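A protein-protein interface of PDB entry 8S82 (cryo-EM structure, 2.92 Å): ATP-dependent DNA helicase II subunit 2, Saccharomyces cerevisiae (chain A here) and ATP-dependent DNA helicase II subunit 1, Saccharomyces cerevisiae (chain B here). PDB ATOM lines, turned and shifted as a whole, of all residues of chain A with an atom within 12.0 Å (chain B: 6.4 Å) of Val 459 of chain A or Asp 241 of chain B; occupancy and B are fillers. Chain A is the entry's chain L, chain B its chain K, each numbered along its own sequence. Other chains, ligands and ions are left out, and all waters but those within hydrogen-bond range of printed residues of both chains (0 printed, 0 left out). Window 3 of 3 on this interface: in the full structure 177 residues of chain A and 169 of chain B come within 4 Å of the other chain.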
ATOM      1  N   PRO A 448     -20.006 -26.460  14.175  1.00  0.00           N
ATOM      2  CA  PRO A 448     -20.803 -25.340  13.660  1.00  0.00           C
ATOM      3  C   PRO A 448     -21.736 -25.764  12.539  1.00  0.00           C
ATOM      4  O   PRO A 448     -21.386 -26.622  11.724  1.00  0.00           O
ATOM      5  CB  PRO A 448     -19.741 -24.350  13.167  1.00  0.00           C
ATOM      6  CG  PRO A 448     -18.513 -25.174  12.970  1.00  0.00           C
ATOM      7  CD  PRO A 448     -18.563 -26.222  14.029  1.00  0.00           C
ATOM      8  N   LYS A 449     -22.927 -25.170  12.492  1.00  0.00           N
ATOM      9  CA  LYS A 449     -23.925 -25.530  11.492  1.00  0.00           C
ATOM     10  C   LYS A 449     -23.425 -25.241  10.083  1.00  0.00           C
ATOM     11  O   LYS A 449     -22.437 -24.525   9.899  1.00  0.00           O
ATOM     12  CB  LYS A 449     -25.238 -24.786  11.752  1.00  0.00           C
ATOM     13  CG  LYS A 449     -26.315 -25.631  12.407  1.00  0.00           C
ATOM     14  CD  LYS A 449     -25.902 -26.079  13.796  1.00  0.00           C
ATOM     15  CE  LYS A 449     -26.864 -27.120  14.345  1.00  0.00           C
ATOM     16  NZ  LYS A 449     -28.268 -26.624  14.371  1.00  0.00           N
ATOM     17  N   LEU A 450     -24.094 -25.808   9.082  1.00  0.00           N
ATOM     18  CA  LEU A 450     -23.692 -25.603   7.698  1.00  0.00           C
ATOM     19  C   LEU A 450     -24.777 -24.879   6.914  1.00  0.00           C
ATOM     20  O   LEU A 450     -24.511 -23.848   6.288  1.00  0.00           O
ATOM     21  CB  LEU A 450     -23.366 -26.942   7.036  1.00  0.00           C
ATOM     22  CG  LEU A 450     -21.887 -27.298   6.886  1.00  0.00           C
ATOM     23  CD1 LEU A 450     -21.151 -27.131   8.204  1.00  0.00           C
ATOM     24  CD2 LEU A 450     -21.749 -28.718   6.369  1.00  0.00           C
ATOM     25  N   LEU A 451     -25.997 -25.414   6.932  1.00  0.00           N
ATOM     26  CA  LEU A 451     -27.078 -24.842   6.138  1.00  0.00           C
ATOM     27  C   LEU A 451     -27.415 -23.431   6.603  1.00  0.00           C
ATOM     28  O   LEU A 451     -27.172 -22.459   5.881  1.00  0.00           O
ATOM     29  CB  LEU A 451     -28.325 -25.730   6.210  1.00  0.00           C
ATOM     30  CG  LEU A 451     -28.219 -27.185   5.740  1.00  0.00           C
ATOM     31  CD1 LEU A 451     -27.678 -28.077   6.840  1.00  0.00           C
ATOM     32  CD2 LEU A 451     -29.565 -27.692   5.260  1.00  0.00           C
ATOM     33  N   ASP A 452     -27.973 -23.310   7.804  1.00  0.00           N
ATOM     34  CA  ASP A 452     -28.214 -22.007   8.422  1.00  0.00           C
ATOM     35  C   ASP A 452     -27.136 -21.700   9.460  1.00  0.00           C
ATOM     36  O   ASP A 452     -27.400 -21.565  10.653  1.00  0.00           O
ATOM     37  CB  ASP A 452     -29.611 -21.966   9.036  1.00  0.00           C
ATOM     38  CG  ASP A 452     -29.914 -23.183   9.883  1.00  0.00           C
ATOM     39  OD1 ASP A 452     -29.610 -23.161  11.094  1.00  0.00           O
ATOM     40  OD2 ASP A 452     -30.457 -24.166   9.336  1.00  0.00           O
ATOM     41  N   ARG A 453     -25.899 -21.582   8.985  1.00  0.00           N
ATOM     42  CA  ARG A 453     -24.781 -21.381   9.896  1.00  0.00           C
ATOM     43  C   ARG A 453     -24.832 -19.987  10.508  1.00  0.00           C
ATOM     44  O   ARG A 453     -25.179 -19.008   9.840  1.00  0.00           O
ATOM     45  CB  ARG A 453     -23.451 -21.609   9.175  1.00  0.00           C
ATOM     46  CG  ARG A 453     -23.066 -20.552   8.163  1.00  0.00           C
ATOM     47  CD  ARG A 453     -21.785 -20.936   7.453  1.00  0.00           C
ATOM     48  NE  ARG A 453     -21.213 -19.818   6.716  1.00  0.00           N
ATOM     49  CZ  ARG A 453     -20.183 -19.095   7.132  1.00  0.00           C
ATOM     50  NH1 ARG A 453     -19.572 -19.359   8.275  1.00  0.00           N
ATOM     51  NH2 ARG A 453     -19.752 -18.086   6.380  1.00  0.00           N
ATOM     52  N   THR A 454     -24.510 -19.908  11.794  1.00  0.00           N
ATOM     53  CA  THR A 454     -24.481 -18.663  12.543  1.00  0.00           C
ATOM     54  C   THR A 454     -23.069 -18.402  13.052  1.00  0.00           C
ATOM     55  O   THR A 454     -22.133 -19.161  12.788  1.00  0.00           O
ATOM     56  CB  THR A 454     -25.464 -18.709  13.718  1.00  0.00           C
ATOM     57  OG1 THR A 454     -24.942 -19.563  14.743  1.00  0.00           O
ATOM     58  CG2 THR A 454     -26.813 -19.249  13.268  1.00  0.00           C
ATOM     59  N   THR A 455     -22.923 -17.306  13.793  1.00  0.00           N
ATOM     60  CA  THR A 455     -21.653 -17.003  14.443  1.00  0.00           C
ATOM     61  C   THR A 455     -21.436 -17.935  15.627  1.00  0.00           C
ATOM     62  O   THR A 455     -22.250 -18.830  15.877  1.00  0.00           O
ATOM     63  CB  THR A 455     -21.604 -15.547  14.912  1.00  0.00           C
ATOM     64  OG1 THR A 455     -22.732 -15.276  15.751  1.00  0.00           O
ATOM     65  CG2 THR A 455     -21.617 -14.599  13.729  1.00  0.00           C
ATOM     66  N   THR A 456     -20.339 -17.735  16.359  1.00  0.00           N
ATOM     67  CA  THR A 456     -20.094 -18.539  17.551  1.00  0.00           C
ATOM     68  C   THR A 456     -21.170 -18.299  18.604  1.00  0.00           C
ATOM     69  O   THR A 456     -21.664 -19.242  19.232  1.00  0.00           O
ATOM     70  CB  THR A 456     -18.708 -18.231  18.115  1.00  0.00           C
ATOM     71  OG1 THR A 456     -17.737 -18.316  17.066  1.00  0.00           O
ATOM     72  CG2 THR A 456     -18.345 -19.228  19.205  1.00  0.00           C
ATOM     73  N   SER A 457     -21.557 -17.037  18.801  1.00  0.00           N
ATOM     74  CA  SER A 457     -22.586 -16.697  19.776  1.00  0.00           C
ATOM     75  C   SER A 457     -23.991 -17.048  19.308  1.00  0.00           C
ATOM     76  O   SER A 457     -24.931 -16.944  20.103  1.00  0.00           O
ATOM     77  CB  SER A 457     -22.520 -15.207  20.115  1.00  0.00           C
ATOM     78  OG  SER A 457     -23.548 -14.845  21.019  1.00  0.00           O
ATOM     79  N   GLY A 458     -24.161 -17.450  18.055  1.00  0.00           N
ATOM     80  CA  GLY A 458     -25.463 -17.810  17.540  1.00  0.00           C
ATOM     81  C   GLY A 458     -26.162 -16.753  16.713  1.00  0.00           C
ATOM     82  O   GLY A 458     -27.372 -16.872  16.495  1.00  0.00           O
ATOM     83  N   VAL A 459     -25.451 -15.736  16.250  1.00  0.00           N
ATOM     84  CA  VAL A 459     -26.021 -14.686  15.409  1.00  0.00           C
ATOM     85  C   VAL A 459     -25.933 -15.145  13.958  1.00  0.00           C
ATOM     86  O   VAL A 459     -24.824 -15.413  13.475  1.00  0.00           O
ATOM     87  CB  VAL A 459     -25.293 -13.344  15.605  1.00  0.00           C
ATOM     88  CG1 VAL A 459     -25.971 -12.250  14.795  1.00  0.00           C
ATOM     89  CG2 VAL A 459     -25.249 -12.977  17.080  1.00  0.00           C
ATOM     90  N   PRO A 460     -27.059 -15.256  13.242  1.00  0.00           N
ATOM     91  CA  PRO A 460     -27.030 -15.799  11.875  1.00  0.00           C
ATOM     92  C   PRO A 460     -26.153 -15.006  10.918  1.00  0.00           C
ATOM     93  O   PRO A 460     -26.083 -13.776  10.991  1.00  0.00           O
ATOM     94  CB  PRO A 460     -28.503 -15.746  11.450  1.00  0.00           C
ATOM     95  CG  PRO A 460     -29.267 -15.779  12.731  1.00  0.00           C
ATOM     96  CD  PRO A 460     -28.432 -15.004  13.709  1.00  0.00           C
ATOM     97  N   LEU A 461     -25.477 -15.715  10.017  1.00  0.00           N
ATOM     98  CA  LEU A 461     -24.592 -15.119   9.019  1.00  0.00           C
ATOM     99  C   LEU A 461     -25.199 -15.362   7.643  1.00  0.00           C
ATOM    100  O   LEU A 461     -25.248 -16.501   7.169  1.00  0.00           O
ATOM    101  CB  LEU A 461     -23.188 -15.708   9.111  1.00  0.00           C
ATOM    102  CG  LEU A 461     -22.316 -15.263  10.282  1.00  0.00           C
ATOM    103  CD1 LEU A 461     -21.014 -16.046  10.302  1.00  0.00           C
ATOM    104  CD2 LEU A 461     -22.043 -13.771  10.197  1.00  0.00           C
ATOM    105  N   LYS A 462     -25.658 -14.289   7.001  1.00  0.00           N
ATOM    106  CA  LYS A 462     -26.224 -14.396   5.662  1.00  0.00           C
ATOM    107  C   LYS A 462     -25.112 -14.603   4.642  1.00  0.00           C
ATOM    108  O   LYS A 462     -24.322 -13.691   4.378  1.00  0.00           O
ATOM    109  CB  LYS A 462     -27.040 -13.148   5.325  1.00  0.00           C
ATOM    110  CG  LYS A 462     -28.050 -12.777   6.396  1.00  0.00           C
ATOM    111  CD  LYS A 462     -28.841 -11.540   6.014  1.00  0.00           C
ATOM    112  CE  LYS A 462     -29.747 -11.103   7.152  1.00  0.00           C
ATOM    113  NZ  LYS A 462     -30.657 -12.199   7.588  1.00  0.00           N
ATOM    114  N   LYS A 463     -25.044 -15.798   4.065  1.00  0.00           N
ATOM    115  CA  LYS A 463     -23.977 -16.155   3.144  1.00  0.00           C
ATOM    116  C   LYS A 463     -24.333 -15.760   1.715  1.00  0.00           C
ATOM    117  O   LYS A 463     -25.472 -15.925   1.268  1.00  0.00           O
ATOM    118  CB  LYS A 463     -23.687 -17.656   3.224  1.00  0.00           C
ATOM    119  CG  LYS A 463     -24.923 -18.535   3.108  1.00  0.00           C
ATOM    120  CD  LYS A 463     -24.805 -19.781   3.972  1.00  0.00           C
ATOM    121  CE  LYS A 463     -23.642 -20.656   3.544  1.00  0.00           C
ATOM    122  NZ  LYS A 463     -23.517 -21.855   4.417  1.00  0.00           N
ATOM    123  N   PHE B 197     -10.019 -13.413  25.624  1.00  0.00           N
ATOM    124  CA  PHE B 197     -10.222 -14.090  24.348  1.00  0.00           C
ATOM    125  C   PHE B 197      -8.964 -14.034  23.493  1.00  0.00           C
ATOM    126  O   PHE B 197      -8.667 -14.966  22.738  1.00  0.00           O
ATOM    127  CB  PHE B 197     -11.409 -13.467  23.613  1.00  0.00           C
ATOM    128  CG  PHE B 197     -11.834 -14.225  22.389  1.00  0.00           C
ATOM    129  CD1 PHE B 197     -11.302 -13.918  21.147  1.00  0.00           C
ATOM    130  CD2 PHE B 197     -12.769 -15.240  22.478  1.00  0.00           C
ATOM    131  CE1 PHE B 197     -11.693 -14.614  20.020  1.00  0.00           C
ATOM    132  CE2 PHE B 197     -13.164 -15.939  21.354  1.00  0.00           C
ATOM    133  CZ  PHE B 197     -12.625 -15.625  20.123  1.00  0.00           C
ATOM    134  N   SER B 221     -24.471 -11.343  27.529  1.00  0.00           N
ATOM    135  CA  SER B 221     -24.348 -11.291  26.076  1.00  0.00           C
ATOM    136  C   SER B 221     -23.570 -10.056  25.644  1.00  0.00           C
ATOM    137  O   SER B 221     -22.752 -10.119  24.720  1.00  0.00           O
ATOM    138  CB  SER B 221     -25.733 -11.313  25.427  1.00  0.00           C
ATOM    139  OG  SER B 221     -25.636 -11.460  24.023  1.00  0.00           O
ATOM    140  N   LEU B 224     -19.625 -10.607  27.174  1.00  0.00           N
ATOM    141  CA  LEU B 224     -18.795 -11.687  26.656  1.00  0.00           C
ATOM    142  C   LEU B 224     -18.525 -11.585  25.161  1.00  0.00           C
ATOM    143  O   LEU B 224     -17.641 -12.289  24.664  1.00  0.00           O
ATOM    144  CB  LEU B 224     -19.443 -13.038  26.965  1.00  0.00           C
ATOM    145  CG  LEU B 224     -19.477 -13.442  28.438  1.00  0.00           C
ATOM    146  CD1 LEU B 224     -20.346 -14.669  28.625  1.00  0.00           C
ATOM    147  CD2 LEU B 224     -18.071 -13.697  28.950  1.00  0.00           C
ATOM    148  N   GLN B 225     -19.247 -10.740  24.435  1.00  0.00           N
ATOM    149  CA  GLN B 225     -18.970 -10.567  23.017  1.00  0.00           C
ATOM    150  C   GLN B 225     -17.793  -9.621  22.822  1.00  0.00           C
ATOM    151  O   GLN B 225     -17.290  -9.013  23.770  1.00  0.00           O
ATOM    152  CB  GLN B 225     -20.206 -10.041  22.285  1.00  0.00           C
ATOM    153  CG  GLN B 225     -20.643  -8.654  22.713  1.00  0.00           C
ATOM    154  CD  GLN B 225     -21.980  -8.261  22.121  1.00  0.00           C
ATOM    155  OE1 GLN B 225     -22.586  -9.022  21.368  1.00  0.00           O
ATOM    156  NE2 GLN B 225     -22.446  -7.065  22.459  1.00  0.00           N
ATOM    157  N   LEU B 226     -17.352  -9.498  21.572  1.00  0.00           N
ATOM    158  CA  LEU B 226     -16.192  -8.687  21.243  1.00  0.00           C
ATOM    159  C   LEU B 226     -16.519  -7.223  20.997  1.00  0.00           C
ATOM    160  O   LEU B 226     -15.771  -6.556  20.272  1.00  0.00           O
ATOM    161  CB  LEU B 226     -15.474  -9.250  20.004  1.00  0.00           C
ATOM    162  CG  LEU B 226     -14.622 -10.511  20.187  1.00  0.00           C
ATOM    163  CD1 LEU B 226     -13.690 -10.357  21.379  1.00  0.00           C
ATOM    164  CD2 LEU B 226     -15.479 -11.765  20.321  1.00  0.00           C
ATOM    165  N   GLY B 227     -17.600  -6.704  21.570  1.00  0.00           N
ATOM    166  CA  GLY B 227     -17.924  -5.305  21.411  1.00  0.00           C
ATOM    167  C   GLY B 227     -18.431  -5.001  20.019  1.00  0.00           C
ATOM    168  O   GLY B 227     -19.000  -5.852  19.328  1.00  0.00           O
ATOM    169  N   SER B 238     -15.573 -10.019  11.872  1.00  0.00           N
ATOM    170  CA  SER B 238     -15.060 -11.098  12.706  1.00  0.00           C
ATOM    171  C   SER B 238     -15.934 -12.339  12.571  1.00  0.00           C
ATOM    172  O   SER B 238     -17.166 -12.248  12.563  1.00  0.00           O
ATOM    173  CB  SER B 238     -14.995 -10.653  14.166  1.00  0.00           C
ATOM    174  OG  SER B 238     -14.145  -9.530  14.320  1.00  0.00           O
ATOM    175  N   GLU B 239     -15.293 -13.499  12.460  1.00  0.00           N
ATOM    176  CA  GLU B 239     -15.988 -14.769  12.306  1.00  0.00           C
ATOM    177  C   GLU B 239     -16.473 -15.345  13.629  1.00  0.00           C
ATOM    178  O   GLU B 239     -17.271 -16.289  13.623  1.00  0.00           O
ATOM    179  CB  GLU B 239     -15.073 -15.783  11.610  1.00  0.00           C
ATOM    180  CG  GLU B 239     -14.441 -15.265  10.329  1.00  0.00           C
ATOM    181  CD  GLU B 239     -13.395 -16.207   9.773  1.00  0.00           C
ATOM    182  OE1 GLU B 239     -13.233 -17.311  10.333  1.00  0.00           O
ATOM    183  OE2 GLU B 239     -12.734 -15.843   8.778  1.00  0.00           O
ATOM    184  N   PHE B 240     -16.016 -14.804  14.754  1.00  0.00           N
ATOM    185  CA  PHE B 240     -16.396 -15.282  16.075  1.00  0.00           C
ATOM    186  C   PHE B 240     -17.135 -14.182  16.824  1.00  0.00           C
ATOM    187  O   PHE B 240     -16.682 -13.034  16.866  1.00  0.00           O
ATOM    188  CB  PHE B 240     -15.167 -15.723  16.876  1.00  0.00           C
ATOM    189  CG  PHE B 240     -14.363 -16.805  16.210  1.00  0.00           C
ATOM    190  CD1 PHE B 240     -14.596 -18.139  16.502  1.00  0.00           C
ATOM    191  CD2 PHE B 240     -13.371 -16.489  15.296  1.00  0.00           C
ATOM    192  CE1 PHE B 240     -13.859 -19.136  15.892  1.00  0.00           C
ATOM    193  CE2 PHE B 240     -12.631 -17.481  14.683  1.00  0.00           C
ATOM    194  CZ  PHE B 240     -12.874 -18.807  14.982  1.00  0.00           C
ATOM    195  N   ASP B 241     -18.277 -14.540  17.421  1.00  0.00           N
ATOM    196  CA  ASP B 241     -19.048 -13.553  18.170  1.00  0.00           C
ATOM    197  C   ASP B 241     -19.022 -13.818  19.673  1.00  0.00           C
ATOM    198  O   ASP B 241     -19.810 -13.209  20.407  1.00  0.00           O
ATOM    199  CB  ASP B 241     -20.501 -13.524  17.669  1.00  0.00           C
ATOM    200  CG  ASP B 241     -21.207 -12.223  17.992  1.00  0.00           C
ATOM    201  OD1 ASP B 241     -20.973 -11.225  17.280  1.00  0.00           O
ATOM    202  OD2 ASP B 241     -21.997 -12.198  18.959  1.00  0.00           O
ATOM    203  N   GLY B 242     -18.144 -14.695  20.153  1.00  0.00           N
ATOM    204  CA  GLY B 242     -18.079 -15.018  21.556  1.00  0.00           C
ATOM    205  C   GLY B 242     -18.914 -16.232  21.909  1.00  0.00           C
ATOM    206  O   GLY B 242     -19.522 -16.870  21.045  1.00  0.00           O
ATOM    207  N   PRO B 243     -18.958 -16.571  23.197  1.00  0.00           N
ATOM    208  CA  PRO B 243     -19.729 -17.743  23.633  1.00  0.00           C
ATOM    209  C   PRO B 243     -21.227 -17.587  23.432  1.00  0.00           C
ATOM    210  O   PRO B 243     -21.749 -16.467  23.425  1.00  0.00           O
ATOM    211  CB  PRO B 243     -19.380 -17.848  25.121  1.00  0.00           C
ATOM    212  CG  PRO B 243     -19.028 -16.459  25.514  1.00  0.00           C
ATOM    213  CD  PRO B 243     -18.322 -15.878  24.328  1.00  0.00           C
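Among the printed residues, pairs that only touch across the chains: Thr 456 of chain A with Phe 240 of chain B (3.2 Å), Thr 456 of chain A with Gly 242 of chain B (3.2 Å), Ser 457 of chain A with Asp 241 of chain B (3.3 Å), Thr 455 of chain A with Asp 241 of chain B (3.4 Å), Thr 456 of chain A with Asp 241 of chain B (3.8 Å) and Val 459 of chain A with Asp 241 of chain B (3.8 Å).
Val 459 of chain A touches just one residue of chain B: Asp 241 (3.8 Å). Of chain A, only Thr 455, Thr 456, Ser 457 and Val 459 come within 4 Å of Asp 241 of chain B. Gln 225 of chain B touches none of the printed residues of chain A. Gly 227 of chain B touches none of the printed residues of chain A. Of chain A, only Thr 456 and Ser 457 come within 4 Å of Gly 242 of chain B. Of the printed residues of chain B, Ser 457 of chain A touches Asp 241 (3.3 Å), Gly 242 (3.0 Å) and Pro 243 (3.4 Å). Of the printed residues of chain B, Thr 455 of chain A touches Asp 241. The nearest residue of chain A that does not touch Asp 241 of chain B is Gly 458 of chain A (5.4 Å).
The side-chain hydroxyl of Ser 457 of chain A lies within hydrogen-bond range of the backbone carbonyl oxygen of Pro 243 of chain B, 3.4 Å away. The backbone NH of Ser 457 of chain A sits at hydrogen-bond distance from the backbone carbonyl oxygen of Gly 242 of chain B (3.0 Å).
N of Val 459 of chain A lies within hydrogen-bond range of OG1 of Thr 455 of chain A (2.8 Å). The side-chain hydroxyl (OG1) of Thr 455 of chain A sits at hydrogen-bond distance from the backbone NH (N) of Gly 458 of chain A (3.5 Å).
Hydrophobic or aromatic side chains of chain A within 4 Å of the printed part of chain B: Val 459. Along chain A the printed residues that touch a printed residue of chain B span positions 455 to 459. Printed residues of chain B that touch a printed residue of chain A: Phe 240, Asp 241, Gly 242 and Pro 243. Hydrophobic or aromatic side chains of chain B that line the printed part of chain A: Phe 240. Among the printed residues, no Asp or Glu carboxylate lies within 4 Å of a Lys or Arg side-chain nitrogen of the other chain.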
